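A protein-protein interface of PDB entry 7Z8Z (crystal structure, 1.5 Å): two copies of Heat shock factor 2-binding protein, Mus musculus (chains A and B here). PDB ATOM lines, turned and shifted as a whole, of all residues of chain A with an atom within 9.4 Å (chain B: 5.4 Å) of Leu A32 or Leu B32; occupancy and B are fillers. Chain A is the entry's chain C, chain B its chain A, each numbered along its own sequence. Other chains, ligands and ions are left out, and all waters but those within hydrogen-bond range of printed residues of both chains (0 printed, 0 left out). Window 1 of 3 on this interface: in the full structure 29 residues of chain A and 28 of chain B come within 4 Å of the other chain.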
ATOM      1  N   ILE A  24      23.818 -13.680 -31.523  1.00  0.00           N
ATOM      2  CA  ILE A  24      23.701 -12.388 -30.850  1.00  0.00           C
ATOM      3  C   ILE A  24      24.210 -12.497 -29.414  1.00  0.00           C
ATOM      4  O   ILE A  24      24.980 -11.654 -28.941  1.00  0.00           O
ATOM      5  CB  ILE A  24      22.248 -11.885 -30.897  1.00  0.00           C
ATOM      6  CG1 ILE A  24      21.769 -11.787 -32.345  1.00  0.00           C
ATOM      7  CG2 ILE A  24      22.146 -10.523 -30.251  1.00  0.00           C
ATOM      8  CD1 ILE A  24      20.308 -11.384 -32.486  1.00  0.00           C
ATOM      9  N   ARG A  25      23.777 -13.538 -28.703  1.00  0.00           N
ATOM     10  CA  ARG A  25      24.337 -13.860 -27.393  1.00  0.00           C
ATOM     11  C   ARG A  25      25.855 -13.807 -27.410  1.00  0.00           C
ATOM     12  O   ARG A  25      26.483 -13.254 -26.497  1.00  0.00           O
ATOM     13  CB  ARG A  25      23.849 -15.248 -26.973  1.00  0.00           C
ATOM     14  CG  ARG A  25      24.514 -15.823 -25.733  1.00  0.00           C
ATOM     15  CD  ARG A  25      24.393 -17.343 -25.701  1.00  0.00           C
ATOM     16  NE  ARG A  25      25.258 -17.962 -26.702  1.00  0.00           N
ATOM     17  CZ  ARG A  25      25.414 -19.270 -26.857  1.00  0.00           C
ATOM     18  NH1 ARG A  25      24.800 -20.138 -26.072  1.00  0.00           N
ATOM     19  NH2 ARG A  25      26.215 -19.718 -27.823  1.00  0.00           N
ATOM     20  N   ASP A  26      26.460 -14.394 -28.441  1.00  0.00           N
ATOM     21  CA  ASP A  26      27.906 -14.581 -28.452  1.00  0.00           C
ATOM     22  C   ASP A  26      28.648 -13.265 -28.653  1.00  0.00           C
ATOM     23  O   ASP A  26      29.670 -13.026 -28.006  1.00  0.00           O
ATOM     24  CB  ASP A  26      28.329 -15.546 -29.565  1.00  0.00           C
ATOM     25  CG  ASP A  26      27.944 -16.988 -29.306  1.00  0.00           C
ATOM     26  OD1 ASP A  26      27.547 -17.323 -28.178  1.00  0.00           O
ATOM     27  OD2 ASP A  26      28.055 -17.793 -30.264  1.00  0.00           O
ATOM     28  N   PHE A  27      28.183 -12.413 -29.568  1.00  0.00           N
ATOM     29  CA  PHE A  27      28.972 -11.254 -29.963  1.00  0.00           C
ATOM     30  C   PHE A  27      28.432  -9.908 -29.497  1.00  0.00           C
ATOM     31  O   PHE A  27      29.217  -8.964 -29.372  1.00  0.00           O
ATOM     32  CB  PHE A  27      29.134 -11.215 -31.492  1.00  0.00           C
ATOM     33  CG  PHE A  27      30.280 -12.044 -31.990  1.00  0.00           C
ATOM     34  CD1 PHE A  27      31.567 -11.541 -31.970  1.00  0.00           C
ATOM     35  CD2 PHE A  27      30.076 -13.333 -32.451  1.00  0.00           C
ATOM     36  CE1 PHE A  27      32.630 -12.308 -32.407  1.00  0.00           C
ATOM     37  CE2 PHE A  27      31.146 -14.098 -32.884  1.00  0.00           C
ATOM     38  CZ  PHE A  27      32.413 -13.579 -32.864  1.00  0.00           C
ATOM     39  N   LEU A  28      27.142  -9.778 -29.217  1.00  0.00           N
ATOM     40  CA  LEU A  28      26.654  -8.456 -28.835  1.00  0.00           C
ATOM     41  C   LEU A  28      27.345  -7.917 -27.586  1.00  0.00           C
ATOM     42  O   LEU A  28      27.724  -6.734 -27.587  1.00  0.00           O
ATOM     43  CB  LEU A  28      25.137  -8.481 -28.656  1.00  0.00           C
ATOM     44  CG  LEU A  28      24.503  -7.105 -28.444  1.00  0.00           C
ATOM     45  CD1 LEU A  28      24.796  -6.134 -29.566  1.00  0.00           C
ATOM     46  CD2 LEU A  28      22.982  -7.248 -28.275  1.00  0.00           C
ATOM     47  N   PRO A  29      27.571  -8.699 -26.522  1.00  0.00           N
ATOM     48  CA  PRO A  29      28.272  -8.145 -25.348  1.00  0.00           C
ATOM     49  C   PRO A  29      29.720  -7.759 -25.616  1.00  0.00           C
ATOM     50  O   PRO A  29      30.314  -7.054 -24.787  1.00  0.00           O
ATOM     51  CB  PRO A  29      28.196  -9.272 -24.311  1.00  0.00           C
ATOM     52  CG  PRO A  29      27.119 -10.200 -24.802  1.00  0.00           C
ATOM     53  CD  PRO A  29      27.102 -10.077 -26.301  1.00  0.00           C
ATOM     54  N   ARG A  30      30.313  -8.217 -26.716  1.00  0.00           N
ATOM     55  CA  ARG A  30      31.665  -7.819 -27.082  1.00  0.00           C
ATOM     56  C   ARG A  30      31.717  -6.451 -27.736  1.00  0.00           C
ATOM     57  O   ARG A  30      32.816  -5.932 -27.956  1.00  0.00           O
ATOM     58  CB  ARG A  30      32.263  -8.884 -27.998  1.00  0.00           C
ATOM     59  CG  ARG A  30      32.294 -10.266 -27.339  1.00  0.00           C
ATOM     60  CD  ARG A  30      32.807 -11.349 -28.259  1.00  0.00           C
ATOM     61  NE  ARG A  30      34.205 -11.155 -28.623  1.00  0.00           N
ATOM     62  CZ  ARG A  30      34.916 -12.024 -29.326  1.00  0.00           C
ATOM     63  NH1 ARG A  30      34.388 -13.148 -29.761  1.00  0.00           N
ATOM     64  NH2 ARG A  30      36.187 -11.749 -29.604  1.00  0.00           N
ATOM     65  N   ILE A  31      30.570  -5.859 -28.048  1.00  0.00           N
ATOM     66  CA  ILE A  31      30.485  -4.462 -28.452  1.00  0.00           C
ATOM     67  C   ILE A  31      29.807  -3.616 -27.381  1.00  0.00           C
ATOM     68  O   ILE A  31      30.299  -2.547 -27.011  1.00  0.00           O
ATOM     69  CB  ILE A  31      29.742  -4.305 -29.796  1.00  0.00           C
ATOM     70  CG1 ILE A  31      30.374  -5.143 -30.885  1.00  0.00           C
ATOM     71  CG2 ILE A  31      29.716  -2.820 -30.189  1.00  0.00           C
ATOM     72  CD1 ILE A  31      29.529  -5.189 -32.148  1.00  0.00           C
ATOM     73  N   LEU A  32      28.651  -4.064 -26.895  1.00  0.00           N
ATOM     74  CA  LEU A  32      27.876  -3.295 -25.926  1.00  0.00           C
ATOM     75  C   LEU A  32      28.440  -3.612 -24.551  1.00  0.00           C
ATOM     76  O   LEU A  32      28.073  -4.596 -23.902  1.00  0.00           O
ATOM     77  CB  LEU A  32      26.394  -3.625 -26.020  1.00  0.00           C
ATOM     78  CG  LEU A  32      25.741  -3.379 -27.382  1.00  0.00           C
ATOM     79  CD1 LEU A  32      24.219  -3.527 -27.262  1.00  0.00           C
ATOM     80  CD2 LEU A  32      26.128  -2.030 -27.928  1.00  0.00           C
ATOM     81  N   ASN A  33      29.364  -2.767 -24.116  1.00  0.00           N
ATOM     82  CA  ASN A  33      29.965  -2.838 -22.797  1.00  0.00           C
ATOM     83  C   ASN A  33      30.424  -1.426 -22.456  1.00  0.00           C
ATOM     84  O   ASN A  33      30.209  -0.481 -23.225  1.00  0.00           O
ATOM     85  CB  ASN A  33      31.105  -3.857 -22.770  1.00  0.00           C
ATOM     86  CG  ASN A  33      32.114  -3.615 -23.856  1.00  0.00           C
ATOM     87  OD1 ASN A  33      32.692  -2.531 -23.940  1.00  0.00           O
ATOM     88  ND2 ASN A  33      32.341  -4.625 -24.694  1.00  0.00           N
ATOM     89  N   GLY A  34      31.065  -1.288 -21.296  1.00  0.00           N
ATOM     90  CA  GLY A  34      31.433   0.023 -20.795  1.00  0.00           C
ATOM     91  C   GLY A  34      32.447   0.765 -21.643  1.00  0.00           C
ATOM     92  O   GLY A  34      32.629   1.973 -21.441  1.00  0.00           O
ATOM     93  N   GLU A  35      33.110   0.088 -22.580  1.00  0.00           N
ATOM     94  CA  GLU A  35      34.149   0.750 -23.358  1.00  0.00           C
ATOM     95  C   GLU A  35      33.583   1.779 -24.327  1.00  0.00           C
ATOM     96  O   GLU A  35      34.303   2.702 -24.717  1.00  0.00           O
ATOM     97  CB  GLU A  35      34.982  -0.290 -24.112  1.00  0.00           C
ATOM     98  CG  GLU A  35      35.724  -1.246 -23.191  1.00  0.00           C
ATOM     99  CD  GLU A  35      36.435  -2.352 -23.941  1.00  0.00           C
ATOM    100  OE1 GLU A  35      36.640  -2.205 -25.165  1.00  0.00           O
ATOM    101  OE2 GLU A  35      36.785  -3.371 -23.308  1.00  0.00           O
ATOM    102  N   LEU A  36      32.313   1.656 -24.714  1.00  0.00           N
ATOM    103  CA  LEU A  36      31.717   2.656 -25.592  1.00  0.00           C
ATOM    104  C   LEU A  36      31.549   3.988 -24.868  1.00  0.00           C
ATOM    105  O   LEU A  36      32.009   5.032 -25.348  1.00  0.00           O
ATOM    106  CB  LEU A  36      30.372   2.159 -26.116  1.00  0.00           C
ATOM    107  CG  LEU A  36      30.385   0.877 -26.943  1.00  0.00           C
ATOM    108  CD1 LEU A  36      28.977   0.552 -27.433  1.00  0.00           C
ATOM    109  CD2 LEU A  36      31.346   0.990 -28.115  1.00  0.00           C
ATOM    110  N   LEU A  37      30.887   3.974 -23.709  1.00  0.00           N
ATOM    111  CA  LEU A  37      30.714   5.209 -22.950  1.00  0.00           C
ATOM    112  C   LEU A  37      32.059   5.763 -22.497  1.00  0.00           C
ATOM    113  O   LEU A  37      32.265   6.982 -22.487  1.00  0.00           O
ATOM    114  CB  LEU A  37      29.806   4.968 -21.747  1.00  0.00           C
ATOM    115  CG  LEU A  37      29.654   6.136 -20.772  1.00  0.00           C
ATOM    116  CD1 LEU A  37      29.056   7.353 -21.457  1.00  0.00           C
ATOM    117  CD2 LEU A  37      28.799   5.721 -19.574  1.00  0.00           C
ATOM    118  N   LEU B  28      18.663  -1.685 -31.737  1.00  0.00           N
ATOM    119  CA  LEU B  28      20.072  -1.995 -31.957  1.00  0.00           C
ATOM    120  C   LEU B  28      20.734  -1.059 -32.961  1.00  0.00           C
ATOM    121  O   LEU B  28      21.868  -0.624 -32.696  1.00  0.00           O
ATOM    122  CB  LEU B  28      20.223  -3.453 -32.384  1.00  0.00           C
ATOM    123  CG  LEU B  28      21.685  -3.912 -32.398  1.00  0.00           C
ATOM    124  CD1 LEU B  28      22.394  -3.723 -31.058  1.00  0.00           C
ATOM    125  CD2 LEU B  28      21.768  -5.365 -32.851  1.00  0.00           C
ATOM    126  N   PRO B  29      20.117  -0.709 -34.097  1.00  0.00           N
ATOM    127  CA  PRO B  29      20.766   0.237 -35.025  1.00  0.00           C
ATOM    128  C   PRO B  29      20.922   1.650 -34.478  1.00  0.00           C
ATOM    129  O   PRO B  29      21.693   2.431 -35.055  1.00  0.00           O
ATOM    130  CB  PRO B  29      19.840   0.234 -36.252  1.00  0.00           C
ATOM    131  CG  PRO B  29      18.979  -0.996 -36.105  1.00  0.00           C
ATOM    132  CD  PRO B  29      18.838  -1.217 -34.623  1.00  0.00           C
ATOM    133  N   ARG B  30      20.229   2.010 -33.401  1.00  0.00           N
ATOM    134  CA  ARG B  30      20.421   3.312 -32.781  1.00  0.00           C
ATOM    135  C   ARG B  30      21.646   3.350 -31.884  1.00  0.00           C
ATOM    136  O   ARG B  30      22.005   4.427 -31.407  1.00  0.00           O
ATOM    137  CB  ARG B  30      19.157   3.686 -32.004  1.00  0.00           C
ATOM    138  CG  ARG B  30      17.903   3.664 -32.889  1.00  0.00           C
ATOM    139  CD  ARG B  30      16.638   3.940 -32.101  1.00  0.00           C
ATOM    140  NE  ARG B  30      16.611   5.284 -31.541  1.00  0.00           N
ATOM    141  CZ  ARG B  30      15.611   5.776 -30.826  1.00  0.00           C
ATOM    142  NH1 ARG B  30      14.519   5.069 -30.586  1.00  0.00           N
ATOM    143  NH2 ARG B  30      15.703   7.014 -30.352  1.00  0.00           N
ATOM    144  N   ILE B  31      22.300   2.214 -31.663  1.00  0.00           N
ATOM    145  CA  ILE B  31      23.611   2.161 -31.026  1.00  0.00           C
ATOM    146  C   ILE B  31      24.689   1.747 -32.018  1.00  0.00           C
ATOM    147  O   ILE B  31      25.761   2.349 -32.075  1.00  0.00           O
ATOM    148  CB  ILE B  31      23.603   1.200 -29.818  1.00  0.00           C
ATOM    149  CG1 ILE B  31      22.465   1.522 -28.865  1.00  0.00           C
ATOM    150  CG2 ILE B  31      24.951   1.264 -29.096  1.00  0.00           C
ATOM    151  CD1 ILE B  31      22.329   0.500 -27.741  1.00  0.00           C
ATOM    152  N   LEU B  32      24.431   0.696 -32.787  1.00  0.00           N
ATOM    153  CA  LEU B  32      25.422   0.157 -33.713  1.00  0.00           C
ATOM    154  C   LEU B  32      25.306   0.945 -35.012  1.00  0.00           C
ATOM    155  O   LEU B  32      24.448   0.665 -35.855  1.00  0.00           O
ATOM    156  CB  LEU B  32      25.220  -1.336 -33.933  1.00  0.00           C
ATOM    157  CG  LEU B  32      25.325  -2.214 -32.689  1.00  0.00           C
ATOM    158  CD1 LEU B  32      25.332  -3.698 -33.109  1.00  0.00           C
ATOM    159  CD2 LEU B  32      26.553  -1.899 -31.869  1.00  0.00           C
ATOM    160  N   ASN B  33      26.178   1.932 -35.167  1.00  0.00           N
ATOM    161  CA  ASN B  33      26.255   2.760 -36.362  1.00  0.00           C
ATOM    162  C   ASN B  33      27.634   3.406 -36.355  1.00  0.00           C
ATOM    163  O   ASN B  33      28.435   3.194 -35.437  1.00  0.00           O
ATOM    164  CB  ASN B  33      25.119   3.783 -36.392  1.00  0.00           C
ATOM    165  CG  ASN B  33      25.066   4.613 -35.145  1.00  0.00           C
ATOM    166  OD1 ASN B  33      26.036   5.277 -34.793  1.00  0.00           O
ATOM    167  ND2 ASN B  33      23.918   4.585 -34.464  1.00  0.00           N
ATOM    168  N   GLY B  34      27.905   4.210 -37.379  1.00  0.00           N
ATOM    169  CA  GLY B  34      29.238   4.753 -37.568  1.00  0.00           C
ATOM    170  C   GLY B  34      29.717   5.663 -36.458  1.00  0.00           C
ATOM    171  O   GLY B  34      30.906   6.007 -36.432  1.00  0.00           O
ATOM    172  N   LEU B  36      30.131   5.062 -33.302  1.00  0.00           N
ATOM    173  CA  LEU B  36      31.043   4.424 -32.358  1.00  0.00           C
ATOM    174  C   LEU B  36      32.483   4.494 -32.855  1.00  0.00           C
ATOM    175  O   LEU B  36      33.376   4.973 -32.146  1.00  0.00           O
ATOM    176  CB  LEU B  36      30.630   2.969 -32.125  1.00  0.00           C
ATOM    177  CG  LEU B  36      29.212   2.741 -31.600  1.00  0.00           C
ATOM    178  CD1 LEU B  36      28.948   1.243 -31.445  1.00  0.00           C
ATOM    179  CD2 LEU B  36      28.973   3.466 -30.291  1.00  0.00           C
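Leu B28 touches its own counterpart, Leu A28.
Ile A31 touches Leu B32, and with the chains exchanged Leu A32 touches Ile B31.
Leu B32 touches its own counterpart, Leu A32.
Of the 4 pairs that touch across the chains among the printed residues, 4 have their exchanged pair printed and touching as well.
Leu A32 touches just these residues of chain B: Ile B31 and Leu B32.
Ile B31 touches just one residue of chain A: Leu A32.
No residue of chain A comes within 4 Å of Asn B33.
Printed residues of chain B within 4 Å of Leu A28: Leu B28.
Of the printed residues of chain A, Leu B28 touches Leu A28 (3.7 Å).
Of the printed residues of chain B, Ile A31 touches Leu B32.
Leu B36 touches none of the printed residues of chain A.
The nearest residue of chain B that does not touch Leu A32 is Leu B28 (4.2 Å).
Of the 8 printed residues of chain B, 3 touch a printed residue of chain A.
Hydrophobic or aromatic side chains of chain B that line the printed part of chain A: Leu B28, Ile B31 and Leu B32.
Hydrophobic or aromatic side chains of chain A that line the printed part of chain B: Leu A28, Ile A31 and Leu A32.
Among the printed residues, 4 pairs touch across the chains.
Among the printed residues, no Asp or Glu carboxylate lies within 4 Å of a Lys or Arg side-chain nitrogen of the other chain.
Leu A28 touches Leu B28.
CG2 of Ile A31 touches CD2 of Leu B32, 3.7 Å away.
CG2 of Ile B31 touches CD2 of Leu A32, 3.7 Å away.
Leu A32 touches Leu B32 (CD2 to CD2, 3.97 Å).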
